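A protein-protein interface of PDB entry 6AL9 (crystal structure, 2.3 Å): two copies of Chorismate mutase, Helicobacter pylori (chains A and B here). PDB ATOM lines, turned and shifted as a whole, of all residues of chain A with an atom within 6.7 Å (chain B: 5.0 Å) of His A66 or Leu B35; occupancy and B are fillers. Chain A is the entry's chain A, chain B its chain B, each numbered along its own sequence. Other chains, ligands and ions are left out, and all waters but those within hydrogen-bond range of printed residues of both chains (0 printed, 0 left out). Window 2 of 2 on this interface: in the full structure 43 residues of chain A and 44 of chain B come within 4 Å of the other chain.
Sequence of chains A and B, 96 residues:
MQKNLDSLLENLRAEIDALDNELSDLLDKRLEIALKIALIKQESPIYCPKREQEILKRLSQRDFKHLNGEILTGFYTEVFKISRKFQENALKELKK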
ATOM      1  N   PHE A  64      35.266 -26.318 -14.190  1.00  0.00           N
ATOM      2  CA  PHE A  64      33.873 -26.203 -14.625  1.00  0.00           C
ATOM      3  C   PHE A  64      33.810 -25.614 -16.032  1.00  0.00           C
ATOM      4  O   PHE A  64      34.604 -24.757 -16.367  1.00  0.00           O
ATOM      5  CB  PHE A  64      33.093 -25.274 -13.698  1.00  0.00           C
ATOM      6  CG  PHE A  64      32.975 -25.763 -12.296  1.00  0.00           C
ATOM      7  CD1 PHE A  64      32.314 -26.947 -12.016  1.00  0.00           C
ATOM      8  CD2 PHE A  64      33.498 -25.032 -11.243  1.00  0.00           C
ATOM      9  CE1 PHE A  64      32.198 -27.400 -10.724  1.00  0.00           C
ATOM     10  CE2 PHE A  64      33.375 -25.484  -9.935  1.00  0.00           C
ATOM     11  CZ  PHE A  64      32.709 -26.662  -9.682  1.00  0.00           C
ATOM     12  N   LYS A  65      32.830 -26.037 -16.828  1.00  0.00           N
ATOM     13  CA  LYS A  65      32.520 -25.360 -18.079  1.00  0.00           C
ATOM     14  C   LYS A  65      32.014 -23.919 -17.876  1.00  0.00           C
ATOM     15  O   LYS A  65      32.418 -23.008 -18.596  1.00  0.00           O
ATOM     16  CB  LYS A  65      31.480 -26.163 -18.861  1.00  0.00           C
ATOM     17  CG  LYS A  65      31.973 -27.524 -19.349  1.00  0.00           C
ATOM     18  CD  LYS A  65      31.159 -28.034 -20.534  1.00  0.00           C
ATOM     19  CE  LYS A  65      31.591 -27.381 -21.849  1.00  0.00           C
ATOM     20  NZ  LYS A  65      30.568 -27.507 -22.935  1.00  0.00           N
ATOM     21  N   HIS A  66      31.118 -23.706 -16.915  1.00  0.00           N
ATOM     22  CA  HIS A  66      30.446 -22.412 -16.827  1.00  0.00           C
ATOM     23  C   HIS A  66      30.514 -21.744 -15.469  1.00  0.00           C
ATOM     24  O   HIS A  66      30.535 -20.511 -15.391  1.00  0.00           O
ATOM     25  CB  HIS A  66      28.977 -22.536 -17.240  1.00  0.00           C
ATOM     26  CG  HIS A  66      28.781 -23.228 -18.544  1.00  0.00           C
ATOM     27  ND1 HIS A  66      29.104 -22.644 -19.749  1.00  0.00           N
ATOM     28  CD2 HIS A  66      28.317 -24.466 -18.834  1.00  0.00           C
ATOM     29  CE1 HIS A  66      28.828 -23.482 -20.728  1.00  0.00           C
ATOM     30  NE2 HIS A  66      28.337 -24.592 -20.201  1.00  0.00           N
ATOM     31  N   LEU A  67      30.526 -22.534 -14.404  1.00  0.00           N
ATOM     32  CA  LEU A  67      30.568 -21.954 -13.071  1.00  0.00           C
ATOM     33  C   LEU A  67      31.837 -21.127 -12.942  1.00  0.00           C
ATOM     34  O   LEU A  67      32.892 -21.521 -13.424  1.00  0.00           O
ATOM     35  CB  LEU A  67      30.581 -23.021 -11.990  1.00  0.00           C
ATOM     36  CG  LEU A  67      29.387 -23.952 -11.843  1.00  0.00           C
ATOM     37  CD1 LEU A  67      29.489 -24.710 -10.515  1.00  0.00           C
ATOM     38  CD2 LEU A  67      28.073 -23.176 -11.926  1.00  0.00           C
ATOM     39  N   ASN A  68      31.714 -19.980 -12.293  1.00  0.00           N
ATOM     40  CA  ASN A  68      32.877 -19.247 -11.817  1.00  0.00           C
ATOM     41  C   ASN A  68      32.636 -18.839 -10.372  1.00  0.00           C
ATOM     42  O   ASN A  68      31.673 -19.299  -9.755  1.00  0.00           O
ATOM     43  CB  ASN A  68      33.109 -18.026 -12.689  1.00  0.00           C
ATOM     44  CG  ASN A  68      31.876 -17.194 -12.825  1.00  0.00           C
ATOM     45  OD1 ASN A  68      31.115 -17.056 -11.877  1.00  0.00           O
ATOM     46  ND2 ASN A  68      31.644 -16.663 -14.011  1.00  0.00           N
ATOM     47  N   ILE A  71      29.221 -17.033  -9.621  1.00  0.00           N
ATOM     48  CA  ILE A  71      28.052 -17.916  -9.679  1.00  0.00           C
ATOM     49  C   ILE A  71      28.004 -18.850  -8.471  1.00  0.00           C
ATOM     50  O   ILE A  71      26.927 -19.120  -7.955  1.00  0.00           O
ATOM     51  CB  ILE A  71      28.033 -18.757 -10.983  1.00  0.00           C
ATOM     52  CG1 ILE A  71      27.817 -17.859 -12.204  1.00  0.00           C
ATOM     53  CG2 ILE A  71      26.978 -19.875 -10.930  1.00  0.00           C
ATOM     54  CD1 ILE A  71      28.058 -18.562 -13.526  1.00  0.00           C
ATOM     55  N   ASP B  28      26.654 -26.996 -12.839  1.00  0.00           N
ATOM     56  CA  ASP B  28      27.401 -26.772 -14.052  1.00  0.00           C
ATOM     57  C   ASP B  28      26.715 -27.385 -15.280  1.00  0.00           C
ATOM     58  O   ASP B  28      26.621 -26.752 -16.327  1.00  0.00           O
ATOM     59  CB  ASP B  28      28.820 -27.326 -13.878  1.00  0.00           C
ATOM     60  CG  ASP B  28      29.825 -26.669 -14.817  1.00  0.00           C
ATOM     61  OD1 ASP B  28      29.788 -25.428 -14.952  1.00  0.00           O
ATOM     62  OD2 ASP B  28      30.662 -27.391 -15.397  1.00  0.00           O
ATOM     63  N   LEU B  31      23.636 -25.431 -16.272  1.00  0.00           N
ATOM     64  CA  LEU B  31      23.957 -24.278 -17.092  1.00  0.00           C
ATOM     65  C   LEU B  31      24.283 -24.648 -18.542  1.00  0.00           C
ATOM     66  O   LEU B  31      24.011 -23.883 -19.448  1.00  0.00           O
ATOM     67  CB  LEU B  31      25.130 -23.524 -16.463  1.00  0.00           C
ATOM     68  CG  LEU B  31      24.827 -22.929 -15.105  1.00  0.00           C
ATOM     69  CD1 LEU B  31      25.950 -21.965 -14.749  1.00  0.00           C
ATOM     70  CD2 LEU B  31      23.450 -22.245 -15.146  1.00  0.00           C
ATOM     71  N   GLU B  32      24.881 -25.810 -18.771  1.00  0.00           N
ATOM     72  CA  GLU B  32      25.164 -26.237 -20.146  1.00  0.00           C
ATOM     73  C   GLU B  32      23.858 -26.486 -20.911  1.00  0.00           C
ATOM     74  O   GLU B  32      23.714 -26.092 -22.074  1.00  0.00           O
ATOM     75  CB  GLU B  32      26.076 -27.467 -20.154  1.00  0.00           C
ATOM     76  CG  GLU B  32      26.067 -28.274 -21.451  1.00  0.00           C
ATOM     77  CD  GLU B  32      26.835 -27.647 -22.615  1.00  0.00           C
ATOM     78  OE1 GLU B  32      27.540 -26.614 -22.412  1.00  0.00           O
ATOM     79  OE2 GLU B  32      26.724 -28.214 -23.747  1.00  0.00           O
ATOM     80  N   ILE B  33      22.897 -27.115 -20.238  1.00  0.00           N
ATOM     81  CA  ILE B  33      21.565 -27.296 -20.810  1.00  0.00           C
ATOM     82  C   ILE B  33      20.862 -25.979 -21.042  1.00  0.00           C
ATOM     83  O   ILE B  33      20.226 -25.791 -22.059  1.00  0.00           O
ATOM     84  CB  ILE B  33      20.662 -28.208 -19.955  1.00  0.00           C
ATOM     85  CG1 ILE B  33      21.231 -29.614 -19.916  1.00  0.00           C
ATOM     86  CG2 ILE B  33      19.265 -28.304 -20.568  1.00  0.00           C
ATOM     87  CD1 ILE B  33      20.585 -30.477 -18.876  1.00  0.00           C
ATOM     88  N   ALA B  34      20.976 -25.065 -20.093  1.00  0.00           N
ATOM     89  CA  ALA B  34      20.372 -23.747 -20.237  1.00  0.00           C
ATOM     90  C   ALA B  34      21.024 -22.965 -21.378  1.00  0.00           C
ATOM     91  O   ALA B  34      20.386 -22.121 -21.997  1.00  0.00           O
ATOM     92  CB  ALA B  34      20.482 -22.969 -18.920  1.00  0.00           C
ATOM     93  N   LEU B  35      22.300 -23.221 -21.620  1.00  0.00           N
ATOM     94  CA  LEU B  35      22.986 -22.613 -22.751  1.00  0.00           C
ATOM     95  C   LEU B  35      22.324 -23.076 -24.047  1.00  0.00           C
ATOM     96  O   LEU B  35      22.001 -22.250 -24.909  1.00  0.00           O
ATOM     97  CB  LEU B  35      24.474 -22.989 -22.779  1.00  0.00           C
ATOM     98  CG  LEU B  35      25.271 -22.360 -23.942  1.00  0.00           C
ATOM     99  CD1 LEU B  35      25.087 -20.850 -24.023  1.00  0.00           C
ATOM    100  CD2 LEU B  35      26.744 -22.697 -23.800  1.00  0.00           C
ATOM    101  N   LYS B  36      22.126 -24.394 -24.166  1.00  0.00           N
ATOM    102  CA  LYS B  36      21.474 -24.946 -25.344  1.00  0.00           C
ATOM    103  C   LYS B  36      20.080 -24.357 -25.540  1.00  0.00           C
ATOM    104  O   LYS B  36      19.719 -24.003 -26.667  1.00  0.00           O
ATOM    105  CB  LYS B  36      21.399 -26.456 -25.260  1.00  0.00           C
ATOM    106  CG  LYS B  36      22.748 -27.126 -25.427  1.00  0.00           C
ATOM    107  CD  LYS B  36      22.815 -28.440 -24.656  1.00  0.00           C
ATOM    108  CE  LYS B  36      23.311 -29.584 -25.512  1.00  0.00           C
ATOM    109  NZ  LYS B  36      24.165 -30.493 -24.702  1.00  0.00           N
ATOM    110  N   ILE B  37      19.307 -24.219 -24.455  1.00  0.00           N
ATOM    111  CA  ILE B  37      17.970 -23.653 -24.555  1.00  0.00           C
ATOM    112  C   ILE B  37      18.024 -22.211 -25.024  1.00  0.00           C
ATOM    113  O   ILE B  37      17.241 -21.809 -25.874  1.00  0.00           O
ATOM    114  CB  ILE B  37      17.198 -23.732 -23.225  1.00  0.00           C
ATOM    115  CG1 ILE B  37      16.750 -25.168 -22.933  1.00  0.00           C
ATOM    116  CG2 ILE B  37      15.955 -22.843 -23.254  1.00  0.00           C
ATOM    117  CD1 ILE B  37      16.463 -25.398 -21.467  1.00  0.00           C
ATOM    118  N   ALA B  38      18.935 -21.426 -24.470  1.00  0.00           N
ATOM    119  CA  ALA B  38      19.032 -20.019 -24.845  1.00  0.00           C
ATOM    120  C   ALA B  38      19.223 -19.860 -26.319  1.00  0.00           C
ATOM    121  O   ALA B  38      18.620 -18.980 -26.928  1.00  0.00           O
ATOM    122  CB  ALA B  38      20.200 -19.363 -24.138  1.00  0.00           C
ATOM    123  N   LEU B  39      20.082 -20.712 -26.877  1.00  0.00           N
ATOM    124  CA  LEU B  39      20.493 -20.634 -28.277  1.00  0.00           C
ATOM    125  C   LEU B  39      19.392 -21.039 -29.232  1.00  0.00           C
ATOM    126  O   LEU B  39      19.258 -20.420 -30.269  1.00  0.00           O
ATOM    127  CB  LEU B  39      21.722 -21.521 -28.527  1.00  0.00           C
ATOM    128  CG  LEU B  39      23.010 -21.076 -27.831  1.00  0.00           C
ATOM    129  CD1 LEU B  39      24.146 -22.060 -28.085  1.00  0.00           C
ATOM    130  CD2 LEU B  39      23.405 -19.674 -28.263  1.00  0.00           C
ATOM    131  N   PHE B  86      22.973 -16.104 -16.661  1.00  0.00           N
ATOM    132  CA  PHE B  86      23.942 -16.821 -17.466  1.00  0.00           C
ATOM    133  C   PHE B  86      23.516 -16.847 -18.945  1.00  0.00           C
ATOM    134  O   PHE B  86      24.324 -16.545 -19.841  1.00  0.00           O
ATOM    135  CB  PHE B  86      24.134 -18.233 -16.915  1.00  0.00           C
ATOM    136  CG  PHE B  86      24.885 -19.142 -17.837  1.00  0.00           C
ATOM    137  CD1 PHE B  86      26.226 -18.933 -18.085  1.00  0.00           C
ATOM    138  CD2 PHE B  86      24.245 -20.205 -18.453  1.00  0.00           C
ATOM    139  CE1 PHE B  86      26.914 -19.768 -18.939  1.00  0.00           C
ATOM    140  CE2 PHE B  86      24.933 -21.047 -19.302  1.00  0.00           C
ATOM    141  CZ  PHE B  86      26.262 -20.832 -19.543  1.00  0.00           C
ATOM    142  N   GLN B  87      22.242 -17.186 -19.180  1.00  0.00           N
ATOM    143  CA  GLN B  87      21.660 -17.251 -20.522  1.00  0.00           C
ATOM    144  C   GLN B  87      21.705 -15.888 -21.230  1.00  0.00           C
ATOM    145  O   GLN B  87      22.066 -15.799 -22.415  1.00  0.00           O
ATOM    146  CB  GLN B  87      20.209 -17.734 -20.455  1.00  0.00           C
ATOM    147  CG  GLN B  87      20.044 -19.231 -20.278  1.00  0.00           C
ATOM    148  CD  GLN B  87      18.589 -19.641 -20.057  1.00  0.00           C
ATOM    149  OE1 GLN B  87      18.050 -19.475 -18.973  1.00  0.00           O
ATOM    150  NE2 GLN B  87      17.969 -20.193 -21.073  1.00  0.00           N
ATOM    151  N   ALA B  90      25.357 -15.138 -22.079  1.00  0.00           N
ATOM    152  CA  ALA B  90      25.682 -15.949 -23.248  1.00  0.00           C
ATOM    153  C   ALA B  90      25.153 -15.332 -24.548  1.00  0.00           C
ATOM    154  O   ALA B  90      25.899 -15.220 -25.527  1.00  0.00           O
ATOM    155  CB  ALA B  90      25.154 -17.365 -23.079  1.00  0.00           C
ATOM    156  N   LEU B  94      27.457 -13.887 -27.714  1.00  0.00           N
ATOM    157  CA  LEU B  94      27.292 -14.660 -28.953  1.00  0.00           C
ATOM    158  C   LEU B  94      26.127 -14.062 -29.794  1.00  0.00           C
ATOM    159  O   LEU B  94      24.976 -14.503 -29.721  1.00  0.00           O
ATOM    160  CB  LEU B  94      27.105 -16.172 -28.643  1.00  0.00           C
ATOM    161  CG  LEU B  94      28.143 -16.894 -27.737  1.00  0.00           C
ATOM    162  CD1 LEU B  94      27.488 -17.988 -26.898  1.00  0.00           C
ATOM    163  CD2 LEU B  94      29.328 -17.478 -28.505  1.00  0.00           C
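The side-chain carboxylate of Asp B28 lies within hydrogen-bond range of the backbone NH of Lys A65, at 2.9 Å.
The side-chain amino group (NZ) of Lys A65 is in salt-bridge range of the side-chain carboxylate (OE1) of Glu B32 (3.2 Å).
The side-chain carboxylate (OD1) of Asp B28 is in hydrogen-bond range of the backbone NH (N) of His A66 (2.9 Å).
The side-chain carboxylate (OE1) of Glu B32 sits at hydrogen-bond distance from a ring nitrogen (NE2) of His A66 (3.1 Å).
The side-chain carboxylate (OD1) of Asp B28 is in hydrogen-bond range of the backbone NH (N) of Leu A67 (3.0 Å).
Among the printed residues, merely in contact across the chains: His A66 with Phe B86 (3.4 Å), Phe A64 with Asp B28 (3.5 Å), Leu A67 with Leu B31 (3.7 Å), His A66 with Leu B35 (3.8 Å) and His A66 with Leu B31 (3.96 Å).
The side-chain carboxylate of Glu B32 lies within salt-bridge range of the side-chain amino group of Lys B36, at 3.6 Å.
His A66 touches five residues of chain B.
Printed residues of chain B within 4 Å of Leu A67: Asp B28 and Leu B31.
Of the printed residues of chain A, Leu B31 touches His A66 and Leu A67.
Leu B35 touches just one residue of chain A: His A66.
Leu B94 touches none of the printed residues of chain A.
The nearest residue of chain A that does not touch Leu B35 is Lys A65 (6.2 Å).
Of the 6 printed residues of chain A, 4 touch a printed residue of chain B.
Of the 14 printed residues of chain B, 5 touch a printed residue of chain A.
Printed residues of chain B that touch a printed residue of chain A: Asp B28, Leu B31, Glu B32, Leu B35 and Phe B86.
Hydrophobic or aromatic side chains of chain B within 4 Å of the printed part of chain A: Leu B31, Leu B35 and Phe B86.
Among the printed residues, 10 pairs touch across the chains.
No position is printed for both chains.
Of the 10 pairs that touch across the chains among the printed residues, none has its exchanged pair printed and touching as well.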
